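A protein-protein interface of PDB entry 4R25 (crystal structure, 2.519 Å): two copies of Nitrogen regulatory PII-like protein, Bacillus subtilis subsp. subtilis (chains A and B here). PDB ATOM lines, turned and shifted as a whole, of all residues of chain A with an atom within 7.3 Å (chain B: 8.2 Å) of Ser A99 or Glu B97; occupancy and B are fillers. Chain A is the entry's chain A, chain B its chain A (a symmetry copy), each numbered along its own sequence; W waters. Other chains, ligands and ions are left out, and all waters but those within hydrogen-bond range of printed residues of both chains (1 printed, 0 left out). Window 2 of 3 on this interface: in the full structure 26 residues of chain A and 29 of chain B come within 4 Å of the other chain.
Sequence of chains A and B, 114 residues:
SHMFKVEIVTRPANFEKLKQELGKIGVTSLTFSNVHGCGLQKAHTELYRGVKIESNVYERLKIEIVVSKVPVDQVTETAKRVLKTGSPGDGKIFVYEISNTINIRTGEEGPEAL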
ATOM      1  N   MET A   3      -8.345  29.743   3.646  1.00  0.00           N
ATOM      2  CA  MET A   3      -8.401  30.593   4.825  1.00  0.00           C
ATOM      3  C   MET A   3      -7.478  31.768   4.582  1.00  0.00           C
ATOM      4  O   MET A   3      -6.389  31.599   4.051  1.00  0.00           O
ATOM      5  CB  MET A   3      -7.958  29.829   6.068  1.00  0.00           C
ATOM      6  CG  MET A   3      -8.531  28.432   6.161  1.00  0.00           C
ATOM      7  SD  MET A   3      -8.070  27.596   7.685  1.00  0.00           S
ATOM      8  CE  MET A   3      -9.187  28.404   8.831  1.00  0.00           C
ATOM      9  N   TYR A  96      -3.183  37.573   2.957  1.00  0.00           N
ATOM     10  CA  TYR A  96      -2.278  36.434   3.036  1.00  0.00           C
ATOM     11  C   TYR A  96      -3.027  35.110   3.084  1.00  0.00           C
ATOM     12  O   TYR A  96      -4.092  35.007   3.686  1.00  0.00           O
ATOM     13  CB  TYR A  96      -1.456  36.488   4.319  1.00  0.00           C
ATOM     14  CG  TYR A  96      -0.657  37.735   4.537  1.00  0.00           C
ATOM     15  CD1 TYR A  96      -1.192  38.799   5.239  1.00  0.00           C
ATOM     16  CD2 TYR A  96       0.651  37.839   4.078  1.00  0.00           C
ATOM     17  CE1 TYR A  96      -0.467  39.945   5.462  1.00  0.00           C
ATOM     18  CE2 TYR A  96       1.396  38.987   4.298  1.00  0.00           C
ATOM     19  CZ  TYR A  96       0.828  40.040   4.992  1.00  0.00           C
ATOM     20  OH  TYR A  96       1.553  41.192   5.216  1.00  0.00           O
ATOM     21  N   GLU A  97      -2.443  34.081   2.488  1.00  0.00           N
ATOM     22  CA  GLU A  97      -2.958  32.727   2.638  1.00  0.00           C
ATOM     23  C   GLU A  97      -2.585  32.192   4.012  1.00  0.00           C
ATOM     24  O   GLU A  97      -1.505  32.498   4.520  1.00  0.00           O
ATOM     25  CB  GLU A  97      -2.374  31.807   1.561  1.00  0.00           C
ATOM     26  CG  GLU A  97      -3.057  31.916   0.202  1.00  0.00           C
ATOM     27  CD  GLU A  97      -2.251  31.289  -0.926  1.00  0.00           C
ATOM     28  OE1 GLU A  97      -1.119  30.805  -0.692  1.00  0.00           O
ATOM     29  OE2 GLU A  97      -2.760  31.290  -2.059  1.00  0.00           O
ATOM     30  N   ILE A  98      -3.469  31.396   4.612  1.00  0.00           N
ATOM     31  CA  ILE A  98      -3.153  30.704   5.855  1.00  0.00           C
ATOM     32  C   ILE A  98      -3.144  29.196   5.642  1.00  0.00           C
ATOM     33  O   ILE A  98      -4.120  28.628   5.167  1.00  0.00           O
ATOM     34  CB  ILE A  98      -4.177  31.003   6.943  1.00  0.00           C
ATOM     35  CG1 ILE A  98      -4.167  32.484   7.309  1.00  0.00           C
ATOM     36  CG2 ILE A  98      -3.891  30.169   8.178  1.00  0.00           C
ATOM     37  CD1 ILE A  98      -5.135  32.823   8.409  1.00  0.00           C
ATOM     38  N   SER A  99      -2.052  28.541   6.013  1.00  0.00           N
ATOM     39  CA  SER A  99      -1.963  27.091   5.873  1.00  0.00           C
ATOM     40  C   SER A  99      -2.951  26.356   6.772  1.00  0.00           C
ATOM     41  O   SER A  99      -3.419  25.279   6.423  1.00  0.00           O
ATOM     42  CB  SER A  99      -0.542  26.593   6.155  1.00  0.00           C
ATOM     43  OG  SER A  99       0.328  26.892   5.079  1.00  0.00           O
ATOM     44  N   ASN A 100      -3.261  26.930   7.930  1.00  0.00           N
ATOM     45  CA  ASN A 100      -4.145  26.268   8.885  1.00  0.00           C
ATOM     46  C   ASN A 100      -4.511  27.144  10.081  1.00  0.00           C
ATOM     47  O   ASN A 100      -3.806  28.093  10.411  1.00  0.00           O
ATOM     48  CB  ASN A 100      -3.519  24.943   9.358  1.00  0.00           C
ATOM     49  CG  ASN A 100      -4.500  24.058  10.134  1.00  0.00           C
ATOM     50  OD1 ASN A 100      -5.698  24.334  10.208  1.00  0.00           O
ATOM     51  ND2 ASN A 100      -3.985  22.982  10.707  1.00  0.00           N
ATOM     52  N   THR A 101      -5.633  26.819  10.710  1.00  0.00           N
ATOM     53  CA  THR A 101      -6.068  27.474  11.930  1.00  0.00           C
ATOM     54  C   THR A 101      -6.494  26.418  12.937  1.00  0.00           C
ATOM     55  O   THR A 101      -7.024  25.376  12.577  1.00  0.00           O
ATOM     56  CB  THR A 101      -7.259  28.401  11.680  1.00  0.00           C
ATOM     57  OG1 THR A 101      -6.942  29.300  10.615  1.00  0.00           O
ATOM     58  CG2 THR A 101      -7.597  29.196  12.941  1.00  0.00           C
ATOM     59  N   GLY A 110      -8.935  24.016  10.483  1.00  0.00           N
ATOM     60  CA  GLY A 110      -9.559  24.493   9.261  1.00  0.00           C
ATOM     61  C   GLY A 110     -10.640  25.525   9.533  1.00  0.00           C
ATOM     62  O   GLY A 110     -10.759  26.019  10.656  1.00  0.00           O
ATOM     63  N   HIS B   2      10.625  22.921   4.117  1.00  0.00           N
ATOM     64  CA  HIS B   2       9.650  23.984   4.306  1.00  0.00           C
ATOM     65  C   HIS B   2      10.022  24.793   5.541  1.00  0.00           C
ATOM     66  O   HIS B   2      10.774  24.329   6.401  1.00  0.00           O
ATOM     67  CB  HIS B   2       8.250  23.407   4.492  1.00  0.00           C
ATOM     68  N   MET B   3       9.492  26.009   5.625  1.00  0.00           N
ATOM     69  CA  MET B   3       9.651  26.833   6.812  1.00  0.00           C
ATOM     70  C   MET B   3       8.291  27.404   7.154  1.00  0.00           C
ATOM     71  O   MET B   3       7.552  27.812   6.269  1.00  0.00           O
ATOM     72  CB  MET B   3      10.643  27.964   6.560  1.00  0.00           C
ATOM     73  CG  MET B   3      11.887  27.530   5.816  1.00  0.00           C
ATOM     74  SD  MET B   3      13.078  28.862   5.623  1.00  0.00           S
ATOM     75  CE  MET B   3      13.772  28.896   7.276  1.00  0.00           C
ATOM     76  N   PHE B   4       7.957  27.435   8.435  1.00  0.00           N
ATOM     77  CA  PHE B   4       6.639  27.902   8.839  1.00  0.00           C
ATOM     78  C   PHE B   4       6.690  28.926   9.950  1.00  0.00           C
ATOM     79  O   PHE B   4       7.604  28.930  10.771  1.00  0.00           O
ATOM     80  CB  PHE B   4       5.755  26.729   9.281  1.00  0.00           C
ATOM     81  CG  PHE B   4       5.435  25.772   8.182  1.00  0.00           C
ATOM     82  CD1 PHE B   4       6.220  24.648   7.970  1.00  0.00           C
ATOM     83  CD2 PHE B   4       4.357  26.000   7.345  1.00  0.00           C
ATOM     84  CE1 PHE B   4       5.927  23.763   6.944  1.00  0.00           C
ATOM     85  CE2 PHE B   4       4.060  25.120   6.318  1.00  0.00           C
ATOM     86  CZ  PHE B   4       4.845  24.002   6.117  1.00  0.00           C
ATOM     87  N   LYS B   5       5.683  29.789   9.975  1.00  0.00           N
ATOM     88  CA  LYS B   5       5.483  30.666  11.105  1.00  0.00           C
ATOM     89  C   LYS B   5       4.255  30.206  11.865  1.00  0.00           C
ATOM     90  O   LYS B   5       3.165  30.099  11.301  1.00  0.00           O
ATOM     91  CB  LYS B   5       5.311  32.110  10.651  1.00  0.00           C
ATOM     92  CG  LYS B   5       5.088  33.096  11.795  1.00  0.00           C
ATOM     93  CD  LYS B   5       4.368  34.320  11.280  1.00  0.00           C
ATOM     94  CE  LYS B   5       4.835  35.585  11.965  1.00  0.00           C
ATOM     95  NZ  LYS B   5       4.288  36.783  11.265  1.00  0.00           N
ATOM     96  N   VAL B   6       4.434  29.935  13.151  1.00  0.00           N
ATOM     97  CA  VAL B   6       3.315  29.600  14.006  1.00  0.00           C
ATOM     98  C   VAL B   6       2.940  30.814  14.839  1.00  0.00           C
ATOM     99  O   VAL B   6       3.755  31.347  15.588  1.00  0.00           O
ATOM    100  CB  VAL B   6       3.622  28.389  14.909  1.00  0.00           C
ATOM    101  CG1 VAL B   6       2.456  28.105  15.846  1.00  0.00           C
ATOM    102  CG2 VAL B   6       3.921  27.179  14.061  1.00  0.00           C
ATOM    103  N   VAL B  72       6.020  21.612  12.575  1.00  0.00           N
ATOM    104  CA  VAL B  72       4.888  22.454  12.932  1.00  0.00           C
ATOM    105  C   VAL B  72       3.906  21.718  13.838  1.00  0.00           C
ATOM    106  O   VAL B  72       3.501  22.243  14.876  1.00  0.00           O
ATOM    107  CB  VAL B  72       4.135  22.942  11.684  1.00  0.00           C
ATOM    108  CG1 VAL B  72       2.843  23.624  12.082  1.00  0.00           C
ATOM    109  CG2 VAL B  72       4.992  23.890  10.900  1.00  0.00           C
ATOM    110  N   ILE B  93      -4.584  29.486  16.820  1.00  0.00           N
ATOM    111  CA  ILE B  93      -3.235  29.286  16.340  1.00  0.00           C
ATOM    112  C   ILE B  93      -3.275  29.321  14.833  1.00  0.00           C
ATOM    113  O   ILE B  93      -4.028  28.577  14.225  1.00  0.00           O
ATOM    114  CB  ILE B  93      -2.687  27.912  16.754  1.00  0.00           C
ATOM    115  CG1 ILE B  93      -2.663  27.777  18.274  1.00  0.00           C
ATOM    116  CG2 ILE B  93      -1.292  27.683  16.161  1.00  0.00           C
ATOM    117  CD1 ILE B  93      -2.282  26.398  18.732  1.00  0.00           C
ATOM    118  N   PHE B  94      -2.448  30.168  14.230  1.00  0.00           N
ATOM    119  CA  PHE B  94      -2.418  30.280  12.782  1.00  0.00           C
ATOM    120  C   PHE B  94      -1.075  29.848  12.209  1.00  0.00           C
ATOM    121  O   PHE B  94      -0.022  30.180  12.747  1.00  0.00           O
ATOM    122  CB  PHE B  94      -2.758  31.711  12.359  1.00  0.00           C
ATOM    123  CG  PHE B  94      -3.983  32.263  13.032  1.00  0.00           C
ATOM    124  CD1 PHE B  94      -5.249  31.960  12.559  1.00  0.00           C
ATOM    125  CD2 PHE B  94      -3.872  33.074  14.146  1.00  0.00           C
ATOM    126  CE1 PHE B  94      -6.383  32.468  13.177  1.00  0.00           C
ATOM    127  CE2 PHE B  94      -5.000  33.580  14.771  1.00  0.00           C
ATOM    128  CZ  PHE B  94      -6.256  33.281  14.285  1.00  0.00           C
ATOM    129  N   VAL B  95      -1.124  29.099  11.114  1.00  0.00           N
ATOM    130  CA  VAL B  95       0.083  28.626  10.460  1.00  0.00           C
ATOM    131  C   VAL B  95       0.243  29.264   9.074  1.00  0.00           C
ATOM    132  O   VAL B  95      -0.718  29.349   8.308  1.00  0.00           O
ATOM    133  CB  VAL B  95       0.103  27.081  10.377  1.00  0.00           C
ATOM    134  CG1 VAL B  95       1.489  26.577   9.963  1.00  0.00           C
ATOM    135  CG2 VAL B  95      -0.302  26.478  11.726  1.00  0.00           C
ATOM    136  N   TYR B  96       1.458  29.734   8.786  1.00  0.00           N
ATOM    137  CA  TYR B  96       1.791  30.373   7.519  1.00  0.00           C
ATOM    138  C   TYR B  96       3.049  29.784   6.895  1.00  0.00           C
ATOM    139  O   TYR B  96       3.992  29.425   7.593  1.00  0.00           O
ATOM    140  CB  TYR B  96       2.087  31.854   7.724  1.00  0.00           C
ATOM    141  CG  TYR B  96       1.009  32.657   8.382  1.00  0.00           C
ATOM    142  CD1 TYR B  96       0.992  32.820   9.755  1.00  0.00           C
ATOM    143  CD2 TYR B  96       0.026  33.290   7.631  1.00  0.00           C
ATOM    144  CE1 TYR B  96       0.018  33.567  10.374  1.00  0.00           C
ATOM    145  CE2 TYR B  96      -0.960  34.049   8.240  1.00  0.00           C
ATOM    146  CZ  TYR B  96      -0.959  34.182   9.617  1.00  0.00           C
ATOM    147  OH  TYR B  96      -1.936  34.931  10.240  1.00  0.00           O
ATOM    148  N   GLU B  97       3.079  29.732   5.571  1.00  0.00           N
ATOM    149  CA  GLU B  97       4.298  29.381   4.857  1.00  0.00           C
ATOM    150  C   GLU B  97       5.252  30.566   4.870  1.00  0.00           C
ATOM    151  O   GLU B  97       4.811  31.714   4.804  1.00  0.00           O
ATOM    152  CB  GLU B  97       3.980  29.004   3.406  1.00  0.00           C
ATOM    153  CG  GLU B  97       3.465  27.580   3.225  1.00  0.00           C
ATOM    154  CD  GLU B  97       2.820  27.345   1.867  1.00  0.00           C
ATOM    155  OE1 GLU B  97       2.705  28.293   1.056  1.00  0.00           O
ATOM    156  OE2 GLU B  97       2.418  26.196   1.619  1.00  0.00           O
ATOM    157  N   ILE B  98       6.554  30.293   4.953  1.00  0.00           N
ATOM    158  CA  ILE B  98       7.563  31.337   4.818  1.00  0.00           C
ATOM    159  C   ILE B  98       8.411  31.104   3.574  1.00  0.00           C
ATOM    160  O   ILE B  98       8.990  30.037   3.407  1.00  0.00           O
ATOM    161  CB  ILE B  98       8.506  31.366   6.013  1.00  0.00           C
ATOM    162  CG1 ILE B  98       7.755  31.717   7.294  1.00  0.00           C
ATOM    163  CG2 ILE B  98       9.618  32.374   5.780  1.00  0.00           C
ATOM    164  CD1 ILE B  98       8.653  31.798   8.498  1.00  0.00           C
ATOM    165  N   SER B  99       8.506  32.107   2.712  1.00  0.00           N
ATOM    166  CA  SER B  99       9.319  31.987   1.506  1.00  0.00           C
ATOM    167  C   SER B  99      10.806  31.849   1.817  1.00  0.00           C
ATOM    168  O   SER B  99      11.534  31.205   1.072  1.00  0.00           O
ATOM    169  CB  SER B  99       9.098  33.177   0.566  1.00  0.00           C
ATOM    170  OG  SER B  99       7.850  33.080  -0.095  1.00  0.00           O
ATOM    171  N   ASN B 100      11.258  32.460   2.908  1.00  0.00           N
ATOM    172  CA  ASN B 100      12.677  32.441   3.247  1.00  0.00           C
ATOM    173  C   ASN B 100      12.983  33.055   4.612  1.00  0.00           C
ATOM    174  O   ASN B 100      12.208  33.849   5.137  1.00  0.00           O
ATOM    175  CB  ASN B 100      13.497  33.138   2.146  1.00  0.00           C
ATOM    176  CG  ASN B 100      15.005  32.911   2.285  1.00  0.00           C
ATOM    177  OD1 ASN B 100      15.465  32.116   3.103  1.00  0.00           O
ATOM    178  ND2 ASN B 100      15.777  33.612   1.470  1.00  0.00           N
HETATM  179  O   HOH W   1       0.708  31.003   3.819  1.00  0.00           O
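N of Ser A99 is in hydrogen-bond range of O of Val B95 (2.8 Å). The backbone NH of Val B95 sits at hydrogen-bond distance from the backbone carbonyl oxygen of Asn A100, 2.9 Å away.
The backbone carbonyl oxygen (O) of Met A3 lies within hydrogen-bond range of the backbone NH (N) of Ile A98 (3.0 Å). OG1 of Thr A101 sits close to SD of Met A3, at 3.6 Å. OD1 of Asn A100 sits at hydrogen-bond distance from N of Gly A110, at 3.3 Å. The backbone NH of Gly A110 lies within hydrogen-bond range of the backbone carbonyl oxygen of Thr A101, 3.1 Å away. The backbone NH (N) of Lys B5 sits at hydrogen-bond distance from the backbone carbonyl oxygen (O) of Tyr B96, 2.9 Å away.
Among the printed residues, merely in contact across the chains: Glu A97 with Tyr B96 (3.6 Å), Ile A98 with Val B95 (3.3 Å), Ile A98 with Tyr B96 (3.7 Å), Ser A99 with Glu B97 (3.7 Å), Asn A100 with Ile B93 (3.9 Å), Asn A100 with Phe B94 (3.5 Å), Thr A101 with Ile B93 (3.3 Å) and Thr A101 with Phe B94 (3.5 Å).
Of chain B, only Val B95 and Glu B97 come within 4 Å of Ser A99. Of chain A, only Ser A99 (3.7 Å) comes within 4 Å of Glu B97. Of the printed residues of chain B, Ile A98 touches Val B95 and Tyr B96. Of the printed residues of chain A, Phe B94 touches Asn A100 and Thr A101. Of the printed residues of chain A, Ile B93 touches Asn A100 (3.9 Å) and Thr A101 (3.3 Å). Asn B100 touches none of the printed residues of chain A. The nearest residue of chain B that does not touch Ser A99 is Phe B4 (4.3 Å).
Hydrophobic or aromatic side chains of chain A within 4 Å of the printed part of chain B: Ile A98.
Glu A97 touches Tyr B96, but with the chains exchanged Tyr A96 does not touch Glu B97 (7.4 Å). Ile A98 touches Tyr B96, but with the chains exchanged Tyr A96 does not touch Ile B98 (9.5 Å). Ser A99 touches Glu B97, but with the chains exchanged Glu A97 does not touch Ser B99 (9.3 Å). Of the 10 pairs that touch across the chains among the printed residues, none has its exchanged pair printed and touching as well.
Water W1 bridges the backbone carbonyl oxygen (O) of Glu A97 and the backbone NH (N) of Glu B97.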
